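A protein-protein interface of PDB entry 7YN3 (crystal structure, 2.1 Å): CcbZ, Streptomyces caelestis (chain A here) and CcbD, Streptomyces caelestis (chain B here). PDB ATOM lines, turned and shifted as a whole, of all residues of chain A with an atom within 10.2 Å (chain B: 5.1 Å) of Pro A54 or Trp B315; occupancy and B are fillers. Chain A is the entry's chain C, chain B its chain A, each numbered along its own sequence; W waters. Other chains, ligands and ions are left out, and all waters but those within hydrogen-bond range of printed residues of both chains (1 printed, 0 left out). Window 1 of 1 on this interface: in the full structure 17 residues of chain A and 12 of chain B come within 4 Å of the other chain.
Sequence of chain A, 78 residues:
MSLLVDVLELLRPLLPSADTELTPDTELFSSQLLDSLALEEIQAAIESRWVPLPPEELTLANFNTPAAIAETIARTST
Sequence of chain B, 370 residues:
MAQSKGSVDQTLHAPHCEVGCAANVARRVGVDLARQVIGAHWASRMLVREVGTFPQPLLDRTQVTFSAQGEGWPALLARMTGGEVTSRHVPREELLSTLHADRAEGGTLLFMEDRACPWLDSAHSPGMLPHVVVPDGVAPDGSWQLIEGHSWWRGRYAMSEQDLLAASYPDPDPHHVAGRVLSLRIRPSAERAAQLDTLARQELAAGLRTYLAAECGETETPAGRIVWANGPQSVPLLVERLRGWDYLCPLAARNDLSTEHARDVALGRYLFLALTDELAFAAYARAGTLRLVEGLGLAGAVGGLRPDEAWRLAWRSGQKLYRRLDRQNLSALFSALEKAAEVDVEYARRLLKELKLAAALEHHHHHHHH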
ATOM      1  N   LEU A  39       4.104 -30.771  16.833  1.00  0.00           N
ATOM      2  CA  LEU A  39       4.384 -29.599  17.660  1.00  0.00           C
ATOM      3  C   LEU A  39       4.610 -28.360  16.799  1.00  0.00           C
ATOM      4  O   LEU A  39       4.158 -27.266  17.146  1.00  0.00           O
ATOM      5  CB  LEU A  39       5.592 -29.857  18.557  1.00  0.00           C
ATOM      6  CG  LEU A  39       5.891 -28.840  19.668  1.00  0.00           C
ATOM      7  CD1 LEU A  39       4.631 -28.485  20.440  1.00  0.00           C
ATOM      8  CD2 LEU A  39       6.973 -29.364  20.623  1.00  0.00           C
ATOM      9  N   GLU A  40       5.299 -28.518  15.667  1.00  0.00           N
ATOM     10  CA  GLU A  40       5.502 -27.396  14.757  1.00  0.00           C
ATOM     11  C   GLU A  40       4.169 -26.821  14.293  1.00  0.00           C
ATOM     12  O   GLU A  40       3.965 -25.601  14.326  1.00  0.00           O
ATOM     13  CB  GLU A  40       6.350 -27.838  13.558  1.00  0.00           C
ATOM     14  CG  GLU A  40       6.657 -26.744  12.545  1.00  0.00           C
ATOM     15  CD  GLU A  40       7.237 -25.486  13.174  1.00  0.00           C
ATOM     16  OE1 GLU A  40       8.055 -25.591  14.129  1.00  0.00           O
ATOM     17  OE2 GLU A  40       6.874 -24.389  12.697  1.00  0.00           O
ATOM     18  N   ILE A  42       1.268 -26.996  15.766  1.00  0.00           N
ATOM     19  CA  ILE A  42       0.602 -26.316  16.868  1.00  0.00           C
ATOM     20  C   ILE A  42       1.205 -24.930  17.083  1.00  0.00           C
ATOM     21  O   ILE A  42       0.487 -23.919  17.130  1.00  0.00           O
ATOM     22  CB  ILE A  42       0.656 -27.175  18.144  1.00  0.00           C
ATOM     23  CG1 ILE A  42      -0.108 -28.490  17.924  1.00  0.00           C
ATOM     24  CG2 ILE A  42       0.071 -26.419  19.321  1.00  0.00           C
ATOM     25  CD1 ILE A  42       0.167 -29.537  18.981  1.00  0.00           C
ATOM     26  N   GLN A  43       2.534 -24.861  17.215  1.00  0.00           N
ATOM     27  CA  GLN A  43       3.184 -23.567  17.407  1.00  0.00           C
ATOM     28  C   GLN A  43       2.831 -22.615  16.286  1.00  0.00           C
ATOM     29  O   GLN A  43       2.546 -21.441  16.530  1.00  0.00           O
ATOM     30  CB  GLN A  43       4.702 -23.722  17.470  1.00  0.00           C
ATOM     31  CG  GLN A  43       5.257 -24.302  18.754  1.00  0.00           C
ATOM     32  CD  GLN A  43       6.768 -24.514  18.650  1.00  0.00           C
ATOM     33  OE1 GLN A  43       7.248 -25.636  18.434  1.00  0.00           O
ATOM     34  NE2 GLN A  43       7.514 -23.425  18.769  1.00  0.00           N
ATOM     35  N   ALA A  44       2.848 -23.105  15.045  1.00  0.00           N
ATOM     36  CA  ALA A  44       2.541 -22.240  13.913  1.00  0.00           C
ATOM     37  C   ALA A  44       1.083 -21.792  13.946  1.00  0.00           C
ATOM     38  O   ALA A  44       0.778 -20.615  13.718  1.00  0.00           O
ATOM     39  CB  ALA A  44       2.871 -22.957  12.607  1.00  0.00           C
ATOM     40  N   ILE A  46      -0.624 -21.267  16.484  1.00  0.00           N
ATOM     41  CA  ILE A  46      -0.845 -20.343  17.590  1.00  0.00           C
ATOM     42  C   ILE A  46      -0.306 -18.954  17.262  1.00  0.00           C
ATOM     43  O   ILE A  46      -0.939 -17.942  17.584  1.00  0.00           O
ATOM     44  CB  ILE A  46      -0.233 -20.916  18.885  1.00  0.00           C
ATOM     45  CG1 ILE A  46      -1.046 -22.122  19.355  1.00  0.00           C
ATOM     46  CG2 ILE A  46      -0.218 -19.874  19.988  1.00  0.00           C
ATOM     47  CD1 ILE A  46      -0.468 -22.828  20.563  1.00  0.00           C
ATOM     48  N   GLU A  47       0.862 -18.867  16.624  1.00  0.00           N
ATOM     49  CA  GLU A  47       1.376 -17.546  16.284  1.00  0.00           C
ATOM     50  C   GLU A  47       0.616 -16.935  15.114  1.00  0.00           C
ATOM     51  O   GLU A  47       0.588 -15.708  14.974  1.00  0.00           O
ATOM     52  CB  GLU A  47       2.870 -17.626  15.955  1.00  0.00           C
ATOM     53  CG  GLU A  47       3.233 -18.934  15.329  1.00  0.00           C
ATOM     54  CD  GLU A  47       4.712 -19.122  15.095  1.00  0.00           C
ATOM     55  OE1 GLU A  47       5.518 -18.758  15.993  1.00  0.00           O
ATOM     56  OE2 GLU A  47       5.053 -19.646  14.003  1.00  0.00           O
ATOM     57  N   TRP A  50      -3.189 -16.353  17.414  1.00  0.00           N
ATOM     58  CA  TRP A  50      -3.401 -15.816  18.752  1.00  0.00           C
ATOM     59  C   TRP A  50      -2.216 -15.058  19.337  1.00  0.00           C
ATOM     60  O   TRP A  50      -2.371 -13.911  19.765  1.00  0.00           O
ATOM     61  CB  TRP A  50      -3.800 -16.954  19.692  1.00  0.00           C
ATOM     62  CG  TRP A  50      -5.118 -17.553  19.338  1.00  0.00           C
ATOM     63  CD1 TRP A  50      -6.322 -16.920  19.326  1.00  0.00           C
ATOM     64  CD2 TRP A  50      -5.369 -18.902  18.929  1.00  0.00           C
ATOM     65  NE1 TRP A  50      -7.314 -17.789  18.939  1.00  0.00           N
ATOM     66  CE2 TRP A  50      -6.756 -19.013  18.688  1.00  0.00           C
ATOM     67  CE3 TRP A  50      -4.558 -20.029  18.747  1.00  0.00           C
ATOM     68  CZ2 TRP A  50      -7.350 -20.207  18.279  1.00  0.00           C
ATOM     69  CZ3 TRP A  50      -5.146 -21.213  18.342  1.00  0.00           C
ATOM     70  CH2 TRP A  50      -6.529 -21.293  18.110  1.00  0.00           C
ATOM     71  N   VAL A  51      -1.038 -15.675  19.398  1.00  0.00           N
ATOM     72  CA  VAL A  51       0.049 -15.085  20.184  1.00  0.00           C
ATOM     73  C   VAL A  51       1.380 -15.702  19.770  1.00  0.00           C
ATOM     74  O   VAL A  51       1.449 -16.915  19.524  1.00  0.00           O
ATOM     75  CB  VAL A  51      -0.219 -15.269  21.691  1.00  0.00           C
ATOM     76  CG1 VAL A  51      -0.509 -16.732  21.999  1.00  0.00           C
ATOM     77  CG2 VAL A  51       0.937 -14.739  22.540  1.00  0.00           C
ATOM     78  N   PRO A  52       2.445 -14.915  19.632  1.00  0.00           N
ATOM     79  CA  PRO A  52       3.751 -15.510  19.315  1.00  0.00           C
ATOM     80  C   PRO A  52       4.424 -16.076  20.559  1.00  0.00           C
ATOM     81  O   PRO A  52       5.032 -15.321  21.322  1.00  0.00           O
ATOM     82  CB  PRO A  52       4.538 -14.331  18.729  1.00  0.00           C
ATOM     83  CG  PRO A  52       3.921 -13.120  19.409  1.00  0.00           C
ATOM     84  CD  PRO A  52       2.471 -13.440  19.595  1.00  0.00           C
ATOM     85  N   LEU A  53       4.340 -17.387  20.768  1.00  0.00           N
ATOM     86  CA  LEU A  53       4.842 -17.978  22.008  1.00  0.00           C
ATOM     87  C   LEU A  53       6.369 -17.968  22.035  1.00  0.00           C
ATOM     88  O   LEU A  53       7.003 -18.389  21.062  1.00  0.00           O
ATOM     89  CB  LEU A  53       4.314 -19.400  22.150  1.00  0.00           C
ATOM     90  CG  LEU A  53       2.870 -19.496  22.656  1.00  0.00           C
ATOM     91  CD1 LEU A  53       2.494 -20.943  22.937  1.00  0.00           C
ATOM     92  CD2 LEU A  53       2.664 -18.627  23.900  1.00  0.00           C
ATOM     93  N   PRO A  54       6.988 -17.492  23.115  1.00  0.00           N
ATOM     94  CA  PRO A  54       8.458 -17.521  23.224  1.00  0.00           C
ATOM     95  C   PRO A  54       8.949 -18.847  23.781  1.00  0.00           C
ATOM     96  O   PRO A  54       8.148 -19.646  24.288  1.00  0.00           O
ATOM     97  CB  PRO A  54       8.747 -16.366  24.195  1.00  0.00           C
ATOM     98  CG  PRO A  54       7.561 -16.383  25.105  1.00  0.00           C
ATOM     99  CD  PRO A  54       6.370 -16.777  24.245  1.00  0.00           C
ATOM    100  N   PRO A  55      10.263 -19.120  23.707  1.00  0.00           N
ATOM    101  CA  PRO A  55      10.787 -20.387  24.257  1.00  0.00           C
ATOM    102  C   PRO A  55      10.314 -20.677  25.672  1.00  0.00           C
ATOM    103  O   PRO A  55       9.986 -21.823  26.002  1.00  0.00           O
ATOM    104  CB  PRO A  55      12.313 -20.175  24.201  1.00  0.00           C
ATOM    105  CG  PRO A  55      12.502 -19.244  23.024  1.00  0.00           C
ATOM    106  CD  PRO A  55      11.323 -18.303  23.086  1.00  0.00           C
ATOM    107  N   GLU A  56      10.255 -19.636  26.501  1.00  0.00           N
ATOM    108  CA  GLU A  56       9.811 -19.727  27.890  1.00  0.00           C
ATOM    109  C   GLU A  56       8.475 -20.465  28.049  1.00  0.00           C
ATOM    110  O   GLU A  56       8.224 -21.081  29.096  1.00  0.00           O
ATOM    111  CB  GLU A  56       9.729 -18.297  28.442  1.00  0.00           C
ATOM    112  CG  GLU A  56       9.538 -18.151  29.928  1.00  0.00           C
ATOM    113  CD  GLU A  56       8.851 -16.837  30.291  1.00  0.00           C
ATOM    114  OE1 GLU A  56       8.916 -15.872  29.489  1.00  0.00           O
ATOM    115  OE2 GLU A  56       8.230 -16.776  31.376  1.00  0.00           O
ATOM    116  N   GLU A  57       7.608 -20.422  27.030  1.00  0.00           N
ATOM    117  CA  GLU A  57       6.293 -21.049  27.105  1.00  0.00           C
ATOM    118  C   GLU A  57       6.242 -22.440  26.487  1.00  0.00           C
ATOM    119  O   GLU A  57       5.205 -23.105  26.589  1.00  0.00           O
ATOM    120  CB  GLU A  57       5.239 -20.163  26.429  1.00  0.00           C
ATOM    121  CG  GLU A  57       5.066 -18.799  27.067  1.00  0.00           C
ATOM    122  CD  GLU A  57       4.474 -18.869  28.471  1.00  0.00           C
ATOM    123  OE1 GLU A  57       3.934 -19.934  28.848  1.00  0.00           O
ATOM    124  OE2 GLU A  57       4.563 -17.855  29.195  1.00  0.00           O
ATOM    125  N   LEU A  58       7.321 -22.899  25.850  1.00  0.00           N
ATOM    126  CA  LEU A  58       7.351 -24.228  25.252  1.00  0.00           C
ATOM    127  C   LEU A  58       7.794 -25.228  26.317  1.00  0.00           C
ATOM    128  O   LEU A  58       8.964 -25.609  26.424  1.00  0.00           O
ATOM    129  CB  LEU A  58       8.268 -24.253  24.034  1.00  0.00           C
ATOM    130  CG  LEU A  58       7.532 -24.265  22.698  1.00  0.00           C
ATOM    131  CD1 LEU A  58       6.654 -25.517  22.556  1.00  0.00           C
ATOM    132  CD2 LEU A  58       6.691 -22.980  22.561  1.00  0.00           C
ATOM    133  N   THR A  59       6.824 -25.638  27.129  1.00  0.00           N
ATOM    134  CA  THR A  59       7.023 -26.604  28.198  1.00  0.00           C
ATOM    135  C   THR A  59       6.016 -27.733  28.030  1.00  0.00           C
ATOM    136  O   THR A  59       4.890 -27.511  27.579  1.00  0.00           O
ATOM    137  CB  THR A  59       6.838 -25.963  29.587  1.00  0.00           C
ATOM    138  OG1 THR A  59       5.444 -25.788  29.844  1.00  0.00           O
ATOM    139  CG2 THR A  59       7.546 -24.604  29.682  1.00  0.00           C
ATOM    140  N   ASN A  62       2.734 -26.958  29.454  1.00  0.00           N
ATOM    141  CA  ASN A  62       1.820 -26.124  28.686  1.00  0.00           C
ATOM    142  C   ASN A  62       1.205 -26.855  27.511  1.00  0.00           C
ATOM    143  O   ASN A  62       0.100 -26.497  27.091  1.00  0.00           O
ATOM    144  CB  ASN A  62       2.538 -24.875  28.184  1.00  0.00           C
ATOM    145  CG  ASN A  62       2.773 -23.880  29.281  1.00  0.00           C
ATOM    146  OD1 ASN A  62       2.290 -24.063  30.402  1.00  0.00           O
ATOM    147  ND2 ASN A  62       3.521 -22.818  28.982  1.00  0.00           N
ATOM    148  N   PHE A  63       1.879 -27.872  26.972  1.00  0.00           N
ATOM    149  CA  PHE A  63       1.498 -28.430  25.683  1.00  0.00           C
ATOM    150  C   PHE A  63       1.048 -29.882  25.741  1.00  0.00           C
ATOM    151  O   PHE A  63       0.783 -30.469  24.688  1.00  0.00           O
ATOM    152  CB  PHE A  63       2.656 -28.299  24.695  1.00  0.00           C
ATOM    153  CG  PHE A  63       2.760 -26.940  24.078  1.00  0.00           C
ATOM    154  CD1 PHE A  63       3.324 -25.892  24.782  1.00  0.00           C
ATOM    155  CD2 PHE A  63       2.270 -26.707  22.804  1.00  0.00           C
ATOM    156  CE1 PHE A  63       3.410 -24.633  24.224  1.00  0.00           C
ATOM    157  CE2 PHE A  63       2.362 -25.447  22.234  1.00  0.00           C
ATOM    158  CZ  PHE A  63       2.927 -24.409  22.947  1.00  0.00           C
ATOM    159  N   THR A  72      -2.658 -21.967  27.980  1.00  0.00           N
ATOM    160  CA  THR A  72      -1.454 -21.227  27.628  1.00  0.00           C
ATOM    161  C   THR A  72      -1.799 -20.052  26.728  1.00  0.00           C
ATOM    162  O   THR A  72      -1.335 -18.928  26.949  1.00  0.00           O
ATOM    163  CB  THR A  72      -0.441 -22.160  26.962  1.00  0.00           C
ATOM    164  OG1 THR A  72      -0.114 -23.224  27.869  1.00  0.00           O
ATOM    165  CG2 THR A  72       0.845 -21.400  26.586  1.00  0.00           C
ATOM    166  N   ILE A  73      -2.660 -20.287  25.736  1.00  0.00           N
ATOM    167  CA  ILE A  73      -3.067 -19.210  24.837  1.00  0.00           C
ATOM    168  C   ILE A  73      -3.810 -18.124  25.610  1.00  0.00           C
ATOM    169  O   ILE A  73      -3.506 -16.930  25.491  1.00  0.00           O
ATOM    170  CB  ILE A  73      -3.918 -19.773  23.686  1.00  0.00           C
ATOM    171  CG1 ILE A  73      -3.082 -20.746  22.845  1.00  0.00           C
ATOM    172  CG2 ILE A  73      -4.510 -18.628  22.838  1.00  0.00           C
ATOM    173  CD1 ILE A  73      -3.892 -21.739  22.066  1.00  0.00           C
ATOM    174  N   ARG A  75      -3.736 -17.327  28.781  1.00  0.00           N
ATOM    175  CA  ARG A  75      -2.888 -16.610  29.726  1.00  0.00           C
ATOM    176  C   ARG A  75      -1.943 -15.636  29.032  1.00  0.00           C
ATOM    177  O   ARG A  75      -1.588 -14.605  29.611  1.00  0.00           O
ATOM    178  CB  ARG A  75      -2.106 -17.627  30.561  1.00  0.00           C
ATOM    179  CG  ARG A  75      -0.944 -17.055  31.353  1.00  0.00           C
ATOM    180  CD  ARG A  75      -0.273 -18.147  32.170  1.00  0.00           C
ATOM    181  NE  ARG A  75       0.659 -18.917  31.356  1.00  0.00           N
ATOM    182  CZ  ARG A  75       0.467 -20.176  30.988  1.00  0.00           C
ATOM    183  NH1 ARG A  75      -0.614 -20.852  31.355  1.00  0.00           N
ATOM    184  NH2 ARG A  75       1.380 -20.774  30.228  1.00  0.00           N
ATOM    185  N   THR A  76      -1.524 -15.931  27.798  1.00  0.00           N
ATOM    186  CA  THR A  76      -0.467 -15.158  27.153  1.00  0.00           C
ATOM    187  C   THR A  76      -0.963 -14.181  26.093  1.00  0.00           C
ATOM    188  O   THR A  76      -0.188 -13.319  25.664  1.00  0.00           O
ATOM    189  CB  THR A  76       0.570 -16.101  26.506  1.00  0.00           C
ATOM    190  OG1 THR A  76      -0.095 -17.002  25.612  1.00  0.00           O
ATOM    191  CG2 THR A  76       1.322 -16.902  27.562  1.00  0.00           C
ATOM    192  N   SER A  77      -2.208 -14.297  25.651  1.00  0.00           N
ATOM    193  CA  SER A  77      -2.718 -13.488  24.540  1.00  0.00           C
ATOM    194  C   SER A  77      -2.642 -11.992  24.809  1.00  0.00           C
ATOM    195  O   SER A  77      -2.944 -11.548  25.912  1.00  0.00           O
ATOM    196  CB  SER A  77      -4.161 -13.883  24.234  1.00  0.00           C
ATOM    197  OG  SER A  77      -4.190 -15.008  23.370  1.00  0.00           O
ATOM    198  N   THR B 276      19.500 -24.122  16.791  1.00  0.00           N
ATOM    199  CA  THR B 276      18.194 -23.607  17.193  1.00  0.00           C
ATOM    200  C   THR B 276      18.142 -23.380  18.698  1.00  0.00           C
ATOM    201  O   THR B 276      17.590 -22.375  19.162  1.00  0.00           O
ATOM    202  CB  THR B 276      17.097 -24.575  16.742  1.00  0.00           C
ATOM    203  OG1 THR B 276      17.115 -24.664  15.311  1.00  0.00           O
ATOM    204  CG2 THR B 276      15.715 -24.084  17.179  1.00  0.00           C
ATOM    205  N   LEU B 279      19.711 -20.065  19.159  1.00  0.00           N
ATOM    206  CA  LEU B 279      18.785 -18.981  18.831  1.00  0.00           C
ATOM    207  C   LEU B 279      17.797 -18.749  19.969  1.00  0.00           C
ATOM    208  O   LEU B 279      17.569 -17.608  20.382  1.00  0.00           O
ATOM    209  CB  LEU B 279      18.051 -19.290  17.520  1.00  0.00           C
ATOM    210  CG  LEU B 279      19.033 -19.666  16.417  1.00  0.00           C
ATOM    211  CD1 LEU B 279      18.361 -19.944  15.083  1.00  0.00           C
ATOM    212  CD2 LEU B 279      20.079 -18.593  16.274  1.00  0.00           C
ATOM    213  N   ALA B 280      17.221 -19.831  20.510  1.00  0.00           N
ATOM    214  CA  ALA B 280      16.360 -19.702  21.684  1.00  0.00           C
ATOM    215  C   ALA B 280      17.082 -19.005  22.833  1.00  0.00           C
ATOM    216  O   ALA B 280      16.488 -18.178  23.537  1.00  0.00           O
ATOM    217  CB  ALA B 280      15.866 -21.081  22.139  1.00  0.00           C
ATOM    218  N   TRP B 311      15.118 -12.399  17.473  1.00  0.00           N
ATOM    219  CA  TRP B 311      15.757 -13.689  17.687  1.00  0.00           C
ATOM    220  C   TRP B 311      14.729 -14.791  17.907  1.00  0.00           C
ATOM    221  O   TRP B 311      14.966 -15.938  17.511  1.00  0.00           O
ATOM    222  CB  TRP B 311      16.734 -13.595  18.854  1.00  0.00           C
ATOM    223  CG  TRP B 311      18.018 -12.943  18.442  1.00  0.00           C
ATOM    224  CD1 TRP B 311      18.421 -11.669  18.709  1.00  0.00           C
ATOM    225  CD2 TRP B 311      19.066 -13.543  17.670  1.00  0.00           C
ATOM    226  NE1 TRP B 311      19.666 -11.434  18.157  1.00  0.00           N
ATOM    227  CE2 TRP B 311      20.076 -12.570  17.504  1.00  0.00           C
ATOM    228  CE3 TRP B 311      19.237 -14.802  17.088  1.00  0.00           C
ATOM    229  CZ2 TRP B 311      21.259 -12.826  16.804  1.00  0.00           C
ATOM    230  CZ3 TRP B 311      20.420 -15.057  16.382  1.00  0.00           C
ATOM    231  CH2 TRP B 311      21.410 -14.072  16.253  1.00  0.00           C
ATOM    232  N   ARG B 312      13.580 -14.464  18.514  1.00  0.00           N
ATOM    233  CA  ARG B 312      12.523 -15.459  18.643  1.00  0.00           C
ATOM    234  C   ARG B 312      12.036 -15.912  17.275  1.00  0.00           C
ATOM    235  O   ARG B 312      11.694 -17.081  17.086  1.00  0.00           O
ATOM    236  CB  ARG B 312      11.361 -14.902  19.465  1.00  0.00           C
ATOM    237  CG  ARG B 312      10.299 -15.931  19.784  1.00  0.00           C
ATOM    238  CD  ARG B 312       8.889 -15.332  19.756  1.00  0.00           C
ATOM    239  NE  ARG B 312       7.909 -16.348  19.393  1.00  0.00           N
ATOM    240  CZ  ARG B 312       7.368 -16.464  18.189  1.00  0.00           C
ATOM    241  NH1 ARG B 312       7.674 -15.618  17.210  1.00  0.00           N
ATOM    242  NH2 ARG B 312       6.491 -17.445  17.962  1.00  0.00           N
ATOM    243  N   LEU B 313      12.013 -15.003  16.301  1.00  0.00           N
ATOM    244  CA  LEU B 313      11.614 -15.400  14.957  1.00  0.00           C
ATOM    245  C   LEU B 313      12.660 -16.317  14.334  1.00  0.00           C
ATOM    246  O   LEU B 313      12.320 -17.331  13.706  1.00  0.00           O
ATOM    247  CB  LEU B 313      11.394 -14.157  14.101  1.00  0.00           C
ATOM    248  CG  LEU B 313      10.024 -13.490  14.302  1.00  0.00           C
ATOM    249  CD1 LEU B 313       9.959 -12.146  13.581  1.00  0.00           C
ATOM    250  CD2 LEU B 313       8.876 -14.397  13.843  1.00  0.00           C
ATOM    251  N   ALA B 314      13.939 -15.974  14.499  1.00  0.00           N
ATOM    252  CA  ALA B 314      15.006 -16.834  14.005  1.00  0.00           C
ATOM    253  C   ALA B 314      14.916 -18.206  14.649  1.00  0.00           C
ATOM    254  O   ALA B 314      15.025 -19.232  13.970  1.00  0.00           O
ATOM    255  CB  ALA B 314      16.365 -16.184  14.282  1.00  0.00           C
ATOM    256  N   TRP B 315      14.651 -18.234  15.961  1.00  0.00           N
ATOM    257  CA  TRP B 315      14.464 -19.490  16.679  1.00  0.00           C
ATOM    258  C   TRP B 315      13.374 -20.341  16.028  1.00  0.00           C
ATOM    259  O   TRP B 315      13.592 -21.520  15.718  1.00  0.00           O
ATOM    260  CB  TRP B 315      14.120 -19.194  18.146  1.00  0.00           C
ATOM    261  CG  TRP B 315      13.551 -20.379  18.911  1.00  0.00           C
ATOM    262  CD1 TRP B 315      14.190 -21.547  19.200  1.00  0.00           C
ATOM    263  CD2 TRP B 315      12.230 -20.494  19.478  1.00  0.00           C
ATOM    264  NE1 TRP B 315      13.344 -22.394  19.905  1.00  0.00           N
ATOM    265  CE2 TRP B 315      12.140 -21.765  20.089  1.00  0.00           C
ATOM    266  CE3 TRP B 315      11.116 -19.655  19.512  1.00  0.00           C
ATOM    267  CZ2 TRP B 315      10.984 -22.204  20.740  1.00  0.00           C
ATOM    268  CZ3 TRP B 315       9.965 -20.090  20.158  1.00  0.00           C
ATOM    269  CH2 TRP B 315       9.908 -21.351  20.764  1.00  0.00           C
ATOM    270  N   ARG B 316      12.191 -19.749  15.798  1.00  0.00           N
ATOM    271  CA  ARG B 316      11.101 -20.503  15.178  1.00  0.00           C
ATOM    272  C   ARG B 316      11.500 -21.014  13.799  1.00  0.00           C
ATOM    273  O   ARG B 316      11.182 -22.154  13.429  1.00  0.00           O
ATOM    274  CB  ARG B 316       9.833 -19.642  15.091  1.00  0.00           C
ATOM    275  CG  ARG B 316       9.131 -19.449  16.445  1.00  0.00           C
ATOM    276  CD  ARG B 316       8.396 -20.708  16.895  1.00  0.00           C
ATOM    277  NE  ARG B 316       7.326 -21.058  15.967  1.00  0.00           N
ATOM    278  CZ  ARG B 316       7.258 -22.188  15.274  1.00  0.00           C
ATOM    279  NH1 ARG B 316       8.170 -23.138  15.410  1.00  0.00           N
ATOM    280  NH2 ARG B 316       6.259 -22.361  14.408  1.00  0.00           N
ATOM    281  N   SER B 317      12.213 -20.193  13.029  1.00  0.00           N
ATOM    282  CA  SER B 317      12.657 -20.636  11.711  1.00  0.00           C
ATOM    283  C   SER B 317      13.636 -21.799  11.811  1.00  0.00           C
ATOM    284  O   SER B 317      13.617 -22.710  10.975  1.00  0.00           O
ATOM    285  CB  SER B 317      13.294 -19.475  10.959  1.00  0.00           C
ATOM    286  OG  SER B 317      12.287 -18.688  10.358  1.00  0.00           O
ATOM    287  N   GLY B 318      14.517 -21.770  12.810  1.00  0.00           N
ATOM    288  CA  GLY B 318      15.408 -22.901  13.016  1.00  0.00           C
ATOM    289  C   GLY B 318      14.657 -24.171  13.365  1.00  0.00           C
ATOM    290  O   GLY B 318      14.981 -25.250  12.864  1.00  0.00           O
ATOM    291  N   GLN B 319      13.645 -24.058  14.227  1.00  0.00           N
ATOM    292  CA  GLN B 319      12.807 -25.205  14.571  1.00  0.00           C
ATOM    293  C   GLN B 319      12.173 -25.825  13.329  1.00  0.00           C
ATOM    294  O   GLN B 319      12.222 -27.043  13.139  1.00  0.00           O
ATOM    295  CB  GLN B 319      11.708 -24.789  15.550  1.00  0.00           C
ATOM    296  CG  GLN B 319      12.173 -24.388  16.940  1.00  0.00           C
ATOM    297  CD  GLN B 319      10.997 -24.258  17.892  1.00  0.00           C
ATOM    298  OE1 GLN B 319      10.087 -23.453  17.661  1.00  0.00           O
ATOM    299  NE2 GLN B 319      11.000 -25.061  18.960  1.00  0.00           N
HETATM  300  O   HOH W   1       8.445 -22.144  12.203  1.00  0.00           O
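Water W1 bridges the side-chain carboxylate (OE2) of Glu A40 and the backbone carbonyl oxygen (O) of Arg B316.
Among the printed residues, merely in contact across the chains: Gln A43 with Trp B315, Ala A44 with Arg B316, Pro A52 with Arg B312, Leu A53 with Trp B315, Pro A54 with Trp B315, Pro A55 with Ala B280 and Pro A55 with Trp B315.
Hydrophobic or aromatic side chains of chain A within 4 Å of the printed part of chain B: Ala A44, Pro A52 and Pro A55. Hydrophobic or aromatic side chains of chain B that line the printed part of chain A: Ala B280 and Trp B315. Along chain B the printed residues that touch a printed residue of chain A span positions 280 to 319. Among the printed residues, 13 pairs touch across the chains. Among the printed residues, Asp or Glu carboxylates within 4 Å of a Lys or Arg side-chain nitrogen of the other chain: Glu A40 with Arg B316 (2.7 Å), Glu A47 with Arg B312 (2.6 Å) and Glu A47 with Arg B316 (2.9 Å).
Printed residues of chain B within 4 Å of Ala A44: Arg B316 (3.5 Å). Of the printed residues of chain B, Pro A54 touches Trp B315. Glu A57 touches none of the printed residues of chain B. Leu B279 touches none of the printed residues of chain A. Ala B280 touches just one residue of chain A: Pro A55 (3.9 Å). Of the printed residues of chain A, Arg B312 touches Glu A47 (2.6 Å), Pro A52 (3.6 Å) and Leu A53 (2.8 Å). No residue of chain A comes within 4 Å of Ala B314. Of the printed residues of chain A, Trp B315 touches Gln A43 (3.7 Å), Leu A53 (3.5 Å), Pro A54 (3.96 Å) and Pro A55 (3.7 Å). No residue of chain A comes within 4 Å of Ser B317. No residue of chain A comes within 4 Å of Gly B318. The nearest printed residue of chain B that does not touch Pro A54 is Arg B312 (4.001 Å). The nearest residue of chain A that does not touch Trp B315 is Leu A58 (4.03 Å). The nearest printed residue of chain B that does not touch Glu A47 is Leu B313 (5.9 Å).
The guanidinium group (NH2) of Arg B312 lies within salt-bridge range of the side-chain carboxylate (OE1) of Glu A47 (2.6 Å). The guanidinium group (NE) of Arg B312 sits at hydrogen-bond distance from the backbone carbonyl oxygen (O) of Leu A53, 2.8 Å away. The guanidinium group (NH2) of Arg B316 lies within salt-bridge range of the side-chain carboxylate (OE2) of Glu A40 (2.7 Å). The side-chain amide nitrogen (NE2) of Gln A43 sits close to the guanidinium group (NH1) of Arg B316, at 3.4 Å. NE of Arg B316 lies within salt-bridge range of OE1 of Glu A47, 2.9 Å away. The side-chain amide oxygen (OE1) of Gln B319 is in hydrogen-bond range of the side-chain amide nitrogen (NE2) of Gln A43 (2.8 Å).
The side-chain amide oxygen of Gln B319 lies within hydrogen-bond range of the guanidinium group of Arg B316 (3.0 Å).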
